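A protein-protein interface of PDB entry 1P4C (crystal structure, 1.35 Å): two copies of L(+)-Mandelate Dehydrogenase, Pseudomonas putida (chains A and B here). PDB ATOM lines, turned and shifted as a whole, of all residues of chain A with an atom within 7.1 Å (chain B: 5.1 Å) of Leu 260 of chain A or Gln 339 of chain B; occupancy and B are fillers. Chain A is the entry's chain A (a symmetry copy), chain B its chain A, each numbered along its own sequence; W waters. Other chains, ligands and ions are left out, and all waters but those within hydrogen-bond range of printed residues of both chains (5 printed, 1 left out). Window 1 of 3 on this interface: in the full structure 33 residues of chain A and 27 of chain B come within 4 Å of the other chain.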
ATOM      1  N   ALA A  31       7.546 -17.747  10.963  1.00  0.00           N
ATOM      2  CA  ALA A  31       6.617 -17.714   9.856  1.00  0.00           C
ATOM      3  C   ALA A  31       5.270 -18.299  10.243  1.00  0.00           C
ATOM      4  O   ALA A  31       5.174 -19.257  11.006  1.00  0.00           O
ATOM      5  CB  ALA A  31       7.185 -18.482   8.672  1.00  0.00           C
ATOM      6  N   GLU A  32       4.230 -17.672   9.725  1.00  0.00           N
ATOM      7  CA  GLU A  32       2.864 -18.110   9.914  1.00  0.00           C
ATOM      8  C   GLU A  32       2.440 -18.595  11.297  1.00  0.00           C
ATOM      9  O   GLU A  32       2.494 -17.826  12.247  1.00  0.00           O
ATOM     10  CB  GLU A  32       2.563 -19.135   8.829  1.00  0.00           C
ATOM     11  CG  GLU A  32       2.967 -18.562   7.467  1.00  0.00           C
ATOM     12  CD  GLU A  32       2.330 -19.270   6.308  1.00  0.00           C
ATOM     13  OE1 GLU A  32       2.265 -20.512   6.335  1.00  0.00           O
ATOM     14  OE2 GLU A  32       1.898 -18.589   5.355  1.00  0.00           O
ATOM     15  N   GLY A  36       6.810 -23.984  13.350  1.00  0.00           N
ATOM     16  CA  GLY A  36       8.202 -24.253  13.035  1.00  0.00           C
ATOM     17  C   GLY A  36       9.149 -23.926  14.169  1.00  0.00           C
ATOM     18  O   GLY A  36       9.981 -24.757  14.540  1.00  0.00           O
ATOM     19  N   VAL A  37       9.048 -22.725  14.730  1.00  0.00           N
ATOM     20  CA  VAL A  37       9.933 -22.391  15.837  1.00  0.00           C
ATOM     21  C   VAL A  37       9.700 -23.356  16.993  1.00  0.00           C
ATOM     22  O   VAL A  37      10.644 -23.738  17.681  1.00  0.00           O
ATOM     23  CB  VAL A  37       9.751 -20.928  16.337  1.00  0.00           C
ATOM     24  CG1 VAL A  37      10.313 -19.955  15.308  1.00  0.00           C
ATOM     25  CG2 VAL A  37       8.286 -20.631  16.618  1.00  0.00           C
ATOM     26  N   THR A 157      20.974 -19.344   1.309  1.00  0.00           N
ATOM     27  CA  THR A 157      20.106 -19.712   0.201  1.00  0.00           C
ATOM     28  C   THR A 157      18.626 -19.887   0.508  1.00  0.00           C
ATOM     29  O   THR A 157      17.856 -20.236  -0.389  1.00  0.00           O
ATOM     30  CB  THR A 157      20.587 -21.037  -0.419  1.00  0.00           C
ATOM     31  OG1 THR A 157      20.429 -22.095   0.541  1.00  0.00           O
ATOM     32  CG2 THR A 157      22.055 -20.942  -0.810  1.00  0.00           C
ATOM     33  N   ASP A 158      18.211 -19.646   1.747  1.00  0.00           N
ATOM     34  CA  ASP A 158      16.808 -19.857   2.078  1.00  0.00           C
ATOM     35  C   ASP A 158      15.894 -18.645   2.157  1.00  0.00           C
ATOM     36  O   ASP A 158      14.906 -18.656   2.891  1.00  0.00           O
ATOM     37  CB  ASP A 158      16.681 -20.686   3.362  1.00  0.00           C
ATOM     38  CG  ASP A 158      17.386 -20.062   4.547  1.00  0.00           C
ATOM     39  OD1 ASP A 158      17.858 -18.908   4.444  1.00  0.00           O
ATOM     40  OD2 ASP A 158      17.459 -20.736   5.599  1.00  0.00           O
ATOM     41  N   VAL A 159      16.211 -17.601   1.400  1.00  0.00           N
ATOM     42  CA  VAL A 159      15.359 -16.418   1.380  1.00  0.00           C
ATOM     43  C   VAL A 159      15.149 -15.973  -0.067  1.00  0.00           C
ATOM     44  O   VAL A 159      15.305 -14.796  -0.397  1.00  0.00           O
ATOM     45  CB  VAL A 159      15.957 -15.253   2.207  1.00  0.00           C
ATOM     46  CG1 VAL A 159      14.902 -14.162   2.396  1.00  0.00           C
ATOM     47  CG2 VAL A 159      16.423 -15.758   3.569  1.00  0.00           C
ATOM     48  N   ALA A 160      14.801 -16.929  -0.926  1.00  0.00           N
ATOM     49  CA  ALA A 160      14.548 -16.652  -2.340  1.00  0.00           C
ATOM     50  C   ALA A 160      13.391 -15.663  -2.412  1.00  0.00           C
ATOM     51  O   ALA A 160      13.318 -14.832  -3.318  1.00  0.00           O
ATOM     52  CB  ALA A 160      14.201 -17.938  -3.074  1.00  0.00           C
ATOM     53  N   VAL A 161      12.481 -15.787  -1.453  1.00  0.00           N
ATOM     54  CA  VAL A 161      11.338 -14.893  -1.306  1.00  0.00           C
ATOM     55  C   VAL A 161      11.255 -14.663   0.199  1.00  0.00           C
ATOM     56  O   VAL A 161      11.806 -15.443   0.976  1.00  0.00           O
ATOM     57  CB  VAL A 161      10.010 -15.507  -1.827  1.00  0.00           C
ATOM     58  CG1 VAL A 161      10.100 -15.744  -3.326  1.00  0.00           C
ATOM     59  CG2 VAL A 161       9.691 -16.796  -1.092  1.00  0.00           C
ATOM     60  N   ASN A 162      10.589 -13.597   0.615  1.00  0.00           N
ATOM     61  CA  ASN A 162      10.491 -13.284   2.032  1.00  0.00           C
ATOM     62  C   ASN A 162       9.499 -14.167   2.783  1.00  0.00           C
ATOM     63  O   ASN A 162       8.430 -14.502   2.269  1.00  0.00           O
ATOM     64  CB  ASN A 162      10.112 -11.811   2.206  1.00  0.00           C
ATOM     65  CG  ASN A 162      11.149 -10.870   1.614  1.00  0.00           C
ATOM     66  OD1 ASN A 162      10.850  -9.718   1.299  1.00  0.00           O
ATOM     67  ND2 ASN A 162      12.378 -11.355   1.473  1.00  0.00           N
ATOM     68  N   GLY A 163       9.871 -14.542   4.003  1.00  0.00           N
ATOM     69  CA  GLY A 163       8.999 -15.365   4.821  1.00  0.00           C
ATOM     70  C   GLY A 163       7.769 -14.581   5.239  1.00  0.00           C
ATOM     71  O   GLY A 163       7.825 -13.364   5.415  1.00  0.00           O
ATOM     72  N   TYR A 164       6.654 -15.280   5.405  1.00  0.00           N
ATOM     73  CA  TYR A 164       5.404 -14.639   5.790  1.00  0.00           C
ATOM     74  C   TYR A 164       5.304 -14.607   7.310  1.00  0.00           C
ATOM     75  O   TYR A 164       4.699 -15.489   7.922  1.00  0.00           O
ATOM     76  CB  TYR A 164       4.230 -15.419   5.201  1.00  0.00           C
ATOM     77  CG  TYR A 164       2.954 -14.626   5.047  1.00  0.00           C
ATOM     78  CD1 TYR A 164       2.866 -13.581   4.127  1.00  0.00           C
ATOM     79  CD2 TYR A 164       1.820 -14.943   5.793  1.00  0.00           C
ATOM     80  CE1 TYR A 164       1.679 -12.879   3.948  1.00  0.00           C
ATOM     81  CE2 TYR A 164       0.629 -14.245   5.624  1.00  0.00           C
ATOM     82  CZ  TYR A 164       0.564 -13.218   4.698  1.00  0.00           C
ATOM     83  OH  TYR A 164      -0.623 -12.545   4.508  1.00  0.00           O
ATOM     84  N   LEU A 234      18.391 -28.210   3.966  1.00  0.00           N
ATOM     85  CA  LEU A 234      17.547 -29.075   4.774  1.00  0.00           C
ATOM     86  C   LEU A 234      17.462 -30.498   4.228  1.00  0.00           C
ATOM     87  O   LEU A 234      16.452 -31.182   4.385  1.00  0.00           O
ATOM     88  CB  LEU A 234      16.151 -28.460   4.911  1.00  0.00           C
ATOM     89  CG  LEU A 234      16.126 -27.208   5.798  1.00  0.00           C
ATOM     90  CD1 LEU A 234      14.765 -26.535   5.698  1.00  0.00           C
ATOM     91  CD2 LEU A 234      16.453 -27.586   7.244  1.00  0.00           C
ATOM     92  N   ASN A 254      16.952 -23.872   9.070  1.00  0.00           N
ATOM     93  CA  ASN A 254      15.662 -23.465   8.524  1.00  0.00           C
ATOM     94  C   ASN A 254      15.448 -21.989   8.856  1.00  0.00           C
ATOM     95  O   ASN A 254      14.325 -21.498   8.939  1.00  0.00           O
ATOM     96  CB  ASN A 254      14.468 -24.341   8.973  1.00  0.00           C
ATOM     97  CG  ASN A 254      14.256 -24.386  10.471  1.00  0.00           C
ATOM     98  OD1 ASN A 254      14.502 -23.425  11.193  1.00  0.00           O
ATOM     99  ND2 ASN A 254      13.747 -25.521  10.941  1.00  0.00           N
ATOM    100  N   HIS A 255      16.562 -21.287   9.045  1.00  0.00           N
ATOM    101  CA  HIS A 255      16.530 -19.853   9.306  1.00  0.00           C
ATOM    102  C   HIS A 255      15.740 -19.529  10.571  1.00  0.00           C
ATOM    103  O   HIS A 255      15.000 -18.546  10.619  1.00  0.00           O
ATOM    104  CB  HIS A 255      15.910 -19.144   8.096  1.00  0.00           C
ATOM    105  CG  HIS A 255      16.422 -17.757   7.865  1.00  0.00           C
ATOM    106  ND1 HIS A 255      17.294 -17.446   6.844  1.00  0.00           N
ATOM    107  CD2 HIS A 255      16.161 -16.594   8.507  1.00  0.00           C
ATOM    108  CE1 HIS A 255      17.546 -16.150   6.865  1.00  0.00           C
ATOM    109  NE2 HIS A 255      16.872 -15.609   7.864  1.00  0.00           N
ATOM    110  N   GLY A 257      13.120 -20.882  11.847  1.00  0.00           N
ATOM    111  CA  GLY A 257      11.676 -20.944  11.676  1.00  0.00           C
ATOM    112  C   GLY A 257      11.049 -19.670  11.142  1.00  0.00           C
ATOM    113  O   GLY A 257       9.837 -19.479  11.237  1.00  0.00           O
ATOM    114  N   ARG A 258      11.873 -18.806  10.556  1.00  0.00           N
ATOM    115  CA  ARG A 258      11.408 -17.520  10.049  1.00  0.00           C
ATOM    116  C   ARG A 258      11.006 -17.486   8.582  1.00  0.00           C
ATOM    117  O   ARG A 258      10.463 -16.479   8.112  1.00  0.00           O
ATOM    118  CB  ARG A 258      12.487 -16.460  10.295  1.00  0.00           C
ATOM    119  CG  ARG A 258      12.791 -16.234  11.766  1.00  0.00           C
ATOM    120  CD  ARG A 258      14.081 -15.456  11.969  1.00  0.00           C
ATOM    121  NE  ARG A 258      14.008 -14.052  11.567  1.00  0.00           N
ATOM    122  CZ  ARG A 258      13.398 -13.097  12.264  1.00  0.00           C
ATOM    123  NH1 ARG A 258      12.786 -13.384  13.406  1.00  0.00           N
ATOM    124  NH2 ARG A 258      13.444 -11.839  11.840  1.00  0.00           N
ATOM    125  N   GLN A 259      11.250 -18.572   7.858  1.00  0.00           N
ATOM    126  CA  GLN A 259      10.923 -18.585   6.437  1.00  0.00           C
ATOM    127  C   GLN A 259       9.794 -19.512   6.005  1.00  0.00           C
ATOM    128  O   GLN A 259       8.896 -19.090   5.280  1.00  0.00           O
ATOM    129  CB  GLN A 259      12.168 -18.906   5.588  1.00  0.00           C
ATOM    130  CG  GLN A 259      13.304 -17.853   5.594  1.00  0.00           C
ATOM    131  CD  GLN A 259      12.835 -16.403   5.506  1.00  0.00           C
ATOM    132  OE1 GLN A 259      12.073 -16.019   4.623  1.00  0.00           O
ATOM    133  NE2 GLN A 259      13.314 -15.586   6.440  1.00  0.00           N
ATOM    134  N   LEU A 260       9.834 -20.768   6.433  1.00  0.00           N
ATOM    135  CA  LEU A 260       8.820 -21.742   6.042  1.00  0.00           C
ATOM    136  C   LEU A 260       8.387 -22.464   7.306  1.00  0.00           C
ATOM    137  O   LEU A 260       9.126 -23.281   7.846  1.00  0.00           O
ATOM    138  CB  LEU A 260       9.429 -22.719   5.035  1.00  0.00           C
ATOM    139  CG  LEU A 260       8.542 -23.832   4.481  1.00  0.00           C
ATOM    140  CD1 LEU A 260       7.370 -23.236   3.706  1.00  0.00           C
ATOM    141  CD2 LEU A 260       9.382 -24.732   3.581  1.00  0.00           C
ATOM    142  N   ASP A 261       7.177 -22.176   7.767  1.00  0.00           N
ATOM    143  CA  ASP A 261       6.700 -22.757   9.011  1.00  0.00           C
ATOM    144  C   ASP A 261       6.744 -24.275   9.088  1.00  0.00           C
ATOM    145  O   ASP A 261       7.075 -24.829  10.136  1.00  0.00           O
ATOM    146  CB  ASP A 261       5.284 -22.262   9.315  1.00  0.00           C
ATOM    147  CG  ASP A 261       4.944 -22.357  10.789  1.00  0.00           C
ATOM    148  OD1 ASP A 261       5.845 -22.108  11.618  1.00  0.00           O
ATOM    149  OD2 ASP A 261       3.780 -22.658  11.126  1.00  0.00           O
ATOM    150  N   CYS A 262       6.446 -24.946   7.982  1.00  0.00           N
ATOM    151  CA  CYS A 262       6.424 -26.404   7.985  1.00  0.00           C
ATOM    152  C   CYS A 262       7.719 -27.093   7.584  1.00  0.00           C
ATOM    153  O   CYS A 262       7.732 -28.291   7.310  1.00  0.00           O
ATOM    154  CB  CYS A 262       5.272 -26.905   7.114  1.00  0.00           C
ATOM    155  SG  CYS A 262       3.657 -26.411   7.757  1.00  0.00           S
ATOM    156  N   ALA A 263       8.812 -26.341   7.557  1.00  0.00           N
ATOM    157  CA  ALA A 263      10.100 -26.925   7.219  1.00  0.00           C
ATOM    158  C   ALA A 263      10.524 -27.890   8.325  1.00  0.00           C
ATOM    159  O   ALA A 263      10.163 -27.715   9.491  1.00  0.00           O
ATOM    160  CB  ALA A 263      11.149 -25.827   7.068  1.00  0.00           C
ATOM    161  N   ILE A 264      11.269 -28.925   7.958  1.00  0.00           N
ATOM    162  CA  ILE A 264      11.770 -29.845   8.963  1.00  0.00           C
ATOM    163  C   ILE A 264      12.818 -29.080   9.760  1.00  0.00           C
ATOM    164  O   ILE A 264      13.276 -28.005   9.344  1.00  0.00           O
ATOM    165  CB  ILE A 264      12.515 -31.058   8.348  1.00  0.00           C
ATOM    166  CG1 ILE A 264      13.607 -30.573   7.385  1.00  0.00           C
ATOM    167  CG2 ILE A 264      11.532 -31.997   7.677  1.00  0.00           C
ATOM    168  CD1 ILE A 264      14.720 -31.594   7.160  1.00  0.00           C
ATOM    169  N   PHE B  49       8.196 -30.089   5.249  1.00  0.00           N
ATOM    170  CA  PHE B  49       8.877 -29.872   3.979  1.00  0.00           C
ATOM    171  C   PHE B  49      10.385 -30.022   4.030  1.00  0.00           C
ATOM    172  O   PHE B  49      11.021 -29.688   5.030  1.00  0.00           O
ATOM    173  CB  PHE B  49       8.594 -28.464   3.448  1.00  0.00           C
ATOM    174  CG  PHE B  49       7.163 -28.218   3.080  1.00  0.00           C
ATOM    175  CD1 PHE B  49       6.534 -28.997   2.116  1.00  0.00           C
ATOM    176  CD2 PHE B  49       6.456 -27.177   3.672  1.00  0.00           C
ATOM    177  CE1 PHE B  49       5.215 -28.738   1.746  1.00  0.00           C
ATOM    178  CE2 PHE B  49       5.140 -26.909   3.308  1.00  0.00           C
ATOM    179  CZ  PHE B  49       4.519 -27.692   2.343  1.00  0.00           C
ATOM    180  N   PRO B  51      12.850 -28.575   1.560  1.00  0.00           N
ATOM    181  CA  PRO B  51      13.107 -27.717   0.402  1.00  0.00           C
ATOM    182  C   PRO B  51      14.306 -28.138  -0.426  1.00  0.00           C
ATOM    183  O   PRO B  51      15.260 -28.726   0.086  1.00  0.00           O
ATOM    184  CB  PRO B  51      13.335 -26.346   1.031  1.00  0.00           C
ATOM    185  CG  PRO B  51      12.494 -26.386   2.261  1.00  0.00           C
ATOM    186  CD  PRO B  51      12.762 -27.776   2.797  1.00  0.00           C
ATOM    187  N   ARG B  53      17.149 -26.513  -2.400  1.00  0.00           N
ATOM    188  CA  ARG B  53      17.821 -25.224  -2.521  1.00  0.00           C
ATOM    189  C   ARG B  53      18.543 -25.019  -3.841  1.00  0.00           C
ATOM    190  O   ARG B  53      18.773 -25.960  -4.599  1.00  0.00           O
ATOM    191  CB  ARG B  53      18.823 -25.043  -1.377  1.00  0.00           C
ATOM    192  CG  ARG B  53      18.192 -24.960   0.006  1.00  0.00           C
ATOM    193  CD  ARG B  53      17.322 -23.727   0.159  1.00  0.00           C
ATOM    194  NE  ARG B  53      16.625 -23.732   1.441  1.00  0.00           N
ATOM    195  CZ  ARG B  53      15.338 -23.432   1.588  1.00  0.00           C
ATOM    196  NH1 ARG B  53      14.605 -23.098   0.537  1.00  0.00           N
ATOM    197  NH2 ARG B  53      14.783 -23.492   2.789  1.00  0.00           N
ATOM    198  N   ARG B 335       4.257 -18.594  -2.660  1.00  0.00           N
ATOM    199  CA  ARG B 335       5.360 -18.389  -1.727  1.00  0.00           C
ATOM    200  C   ARG B 335       5.945 -19.734  -1.297  1.00  0.00           C
ATOM    201  O   ARG B 335       7.165 -19.909  -1.242  1.00  0.00           O
ATOM    202  CB  ARG B 335       4.844 -17.621  -0.508  1.00  0.00           C
ATOM    203  CG  ARG B 335       5.885 -17.236   0.518  1.00  0.00           C
ATOM    204  CD  ARG B 335       5.241 -16.428   1.641  1.00  0.00           C
ATOM    205  NE  ARG B 335       4.587 -15.218   1.142  1.00  0.00           N
ATOM    206  CZ  ARG B 335       3.272 -15.010   1.133  1.00  0.00           C
ATOM    207  NH1 ARG B 335       2.437 -15.928   1.602  1.00  0.00           N
ATOM    208  NH2 ARG B 335       2.786 -13.875   0.650  1.00  0.00           N
ATOM    209  N   THR B 336       5.065 -20.685  -1.007  1.00  0.00           N
ATOM    210  CA  THR B 336       5.487 -22.010  -0.581  1.00  0.00           C
ATOM    211  C   THR B 336       6.282 -22.717  -1.673  1.00  0.00           C
ATOM    212  O   THR B 336       7.303 -23.346  -1.393  1.00  0.00           O
ATOM    213  CB  THR B 336       4.268 -22.858  -0.182  1.00  0.00           C
ATOM    214  OG1 THR B 336       3.561 -22.193   0.872  1.00  0.00           O
ATOM    215  CG2 THR B 336       4.704 -24.237   0.302  1.00  0.00           C
ATOM    216  N   LEU B 337       5.818 -22.616  -2.914  1.00  0.00           N
ATOM    217  CA  LEU B 337       6.518 -23.240  -4.035  1.00  0.00           C
ATOM    218  C   LEU B 337       7.932 -22.678  -4.149  1.00  0.00           C
ATOM    219  O   LEU B 337       8.891 -23.421  -4.371  1.00  0.00           O
ATOM    220  CB  LEU B 337       5.764 -22.998  -5.346  1.00  0.00           C
ATOM    221  CG  LEU B 337       4.415 -23.702  -5.497  1.00  0.00           C
ATOM    222  CD1 LEU B 337       3.821 -23.369  -6.862  1.00  0.00           C
ATOM    223  CD2 LEU B 337       4.595 -25.204  -5.343  1.00  0.00           C
ATOM    224  N   ALA B 338       8.058 -21.366  -3.997  1.00  0.00           N
ATOM    225  CA  ALA B 338       9.362 -20.724  -4.081  1.00  0.00           C
ATOM    226  C   ALA B 338      10.257 -21.231  -2.959  1.00  0.00           C
ATOM    227  O   ALA B 338      11.417 -21.581  -3.183  1.00  0.00           O
ATOM    228  CB  ALA B 338       9.210 -19.211  -3.980  1.00  0.00           C
ATOM    229  N   GLN B 339       9.705 -21.287  -1.753  1.00  0.00           N
ATOM    230  CA  GLN B 339      10.459 -21.725  -0.586  1.00  0.00           C
ATOM    231  C   GLN B 339      10.908 -23.182  -0.606  1.00  0.00           C
ATOM    232  O   GLN B 339      11.953 -23.506  -0.043  1.00  0.00           O
ATOM    233  CB  GLN B 339       9.650 -21.434   0.678  1.00  0.00           C
ATOM    234  CG  GLN B 339       9.589 -19.945   1.003  1.00  0.00           C
ATOM    235  CD  GLN B 339       8.437 -19.576   1.917  1.00  0.00           C
ATOM    236  OE1 GLN B 339       8.471 -18.545   2.588  1.00  0.00           O
ATOM    237  NE2 GLN B 339       7.401 -20.406   1.932  1.00  0.00           N
ATOM    238  N   ILE B 340      10.141 -24.064  -1.243  1.00  0.00           N
ATOM    239  CA  ILE B 340      10.546 -25.465  -1.290  1.00  0.00           C
ATOM    240  C   ILE B 340      11.305 -25.812  -2.568  1.00  0.00           C
ATOM    241  O   ILE B 340      11.711 -26.953  -2.765  1.00  0.00           O
ATOM    242  CB  ILE B 340       9.344 -26.434  -1.116  1.00  0.00           C
ATOM    243  CG1 ILE B 340       8.386 -26.337  -2.302  1.00  0.00           C
ATOM    244  CG2 ILE B 340       8.623 -26.124   0.195  1.00  0.00           C
ATOM    245  CD1 ILE B 340       7.246 -27.349  -2.234  1.00  0.00           C
ATOM    246  N   GLY B 341      11.495 -24.818  -3.430  1.00  0.00           N
ATOM    247  CA  GLY B 341      12.235 -25.043  -4.659  1.00  0.00           C
ATOM    248  C   GLY B 341      11.518 -25.795  -5.761  1.00  0.00           C
ATOM    249  O   GLY B 341      12.145 -26.550  -6.503  1.00  0.00           O
HETATM  250  O   HOH W   1      17.721 -28.204   1.285  1.00  0.00           O
HETATM  251  O   HOH W   2       6.850 -13.783   0.220  1.00  0.00           O
HETATM  252  O   HOH W   3       2.922 -18.588   2.711  1.00  0.00           O
HETATM  253  O   HOH W   4       6.564 -18.036   4.876  1.00  0.00           O
HETATM  254  O   HOH W   5      16.054 -23.054   5.341  1.00  0.00           O
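Printed residues of chain B within 4 Å of Leu 260 of chain A: Phe 49, Pro 51, Gln 339 and Ile 340. Of chain A, only Val 161 (3.8 Å), Gly 163 (3.9 Å), Gln 259 (2.8 Å) and Leu 260 (3.3 Å) come within 4 Å of Gln 339 of chain B. Of the printed residues of chain A, Phe 49 of chain B touches Leu 260, Cys 262, Ala 263 and Ile 264. Of the printed residues of chain A, Ile 340 of chain B touches Leu 260. Of the printed residues of chain B, Gly 163 of chain A touches Gln 339. The nearest printed residue of chain A that does not touch Pro 51 of chain B is Ala 263 of chain A (5.0 Å).
The guanidinium group (NH1) of Arg 53 of chain B sits at hydrogen-bond distance from the backbone carbonyl oxygen (O) of Gln 339 of chain B, 2.7 Å away. O of Arg 335 of chain B is in hydrogen-bond range of NE2 of Gln 339 of chain B (3.2 Å). The backbone NH of Glu 32 of chain A sits at hydrogen-bond distance from the backbone carbonyl oxygen of Tyr 164 of chain A. ND1 of His 255 of chain A sits at hydrogen-bond distance from OD1 of Asp 158 of chain A (2.9 Å). OE1 of Gln 259 of chain A is in hydrogen-bond range of N of Gly 163 of chain A, at 2.7 Å. ND2 of Asn 254 of chain A sits at hydrogen-bond distance from O of Ile 264 of chain A, 3.0 Å away.
Water W4 lies within hydrogen-bond range of O of Gln 259 of chain A (2.6 Å), N of Tyr 164 of chain A (2.8 Å) and OE1 of Gln 339 of chain B (3.0 Å). Water W2 bridges the backbone carbonyl oxygen (O) of Asn 162 of chain A (2.7 Å) and the guanidinium group (NE) of Arg 335 of chain B (2.8 Å). Water W5 bridges OD2 of Asp 158 of chain A (2.7 Å) and NH2 of Arg 53 of chain B (2.9 Å). Water W1 bridges the backbone NH (N) of Leu 234 of chain A (2.8 Å) and the backbone carbonyl oxygen (O) of Pro 51 of chain B (2.8 Å). Water W3 lies within hydrogen-bond range of OE2 of Glu 32 of chain A (2.8 Å) and NH1 of Arg 335 of chain B (2.9 Å).
No position is printed for both chains.
The backbone carbonyl oxygen of Cys 262 of chain A lies within hydrogen-bond range of the backbone NH of Phe 49 of chain B (2.8 Å). The backbone carbonyl oxygen (O) of Phe 49 of chain B lies within hydrogen-bond range of the backbone NH (N) of Ile 264 of chain A, at 3.0 Å. OE1 of Gln 339 of chain B lies close to O of Gln 259 of chain A, 2.8 Å away.
Of the 10 printed residues of chain B, 7 touch a printed residue of chain A. Hydrophobic or aromatic side chains of chain B that line the printed part of chain A: Phe 49, Pro 51, Ala 338 and Ile 340. Of the 23 printed residues of chain A, 12 touch a printed residue of chain B. Among the printed residues, 16 pairs touch across the chains. Among the printed residues, no Asp or Glu carboxylate lies within 4 Å of a Lys or Arg side-chain nitrogen of the other chain.
Among the printed residues, pairs that only touch across the chains: Thr 157 of chain A with Arg 53 of chain B (3.5 Å), Asp 158 of chain A with Arg 53 of chain B (3.4 Å), Val 161 of chain A with Ala 338 of chain B (3.6 Å), Val 161 of chain A with Gln 339 of chain B (3.8 Å), Asn 162 of chain A with Arg 335 of chain B (3.8 Å), Gly 163 of chain A with Gln 339 of chain B (3.9 Å), Tyr 164 of chain A with Arg 335 of chain B (3.3 Å), Leu 234 of chain A with Pro 51 of chain B (3.7 Å), Leu 260 of chain A with Phe 49 of chain B (3.8 Å), Leu 260 of chain A with Pro 51 of chain B (3.8 Å), Leu 260 of chain A with Gln 339 of chain B (3.3 Å), Leu 260 of chain A with Ile 340 of chain B (3.7 Å) and Ala 263 of chain A with Phe 49 of chain B (3.6 Å).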
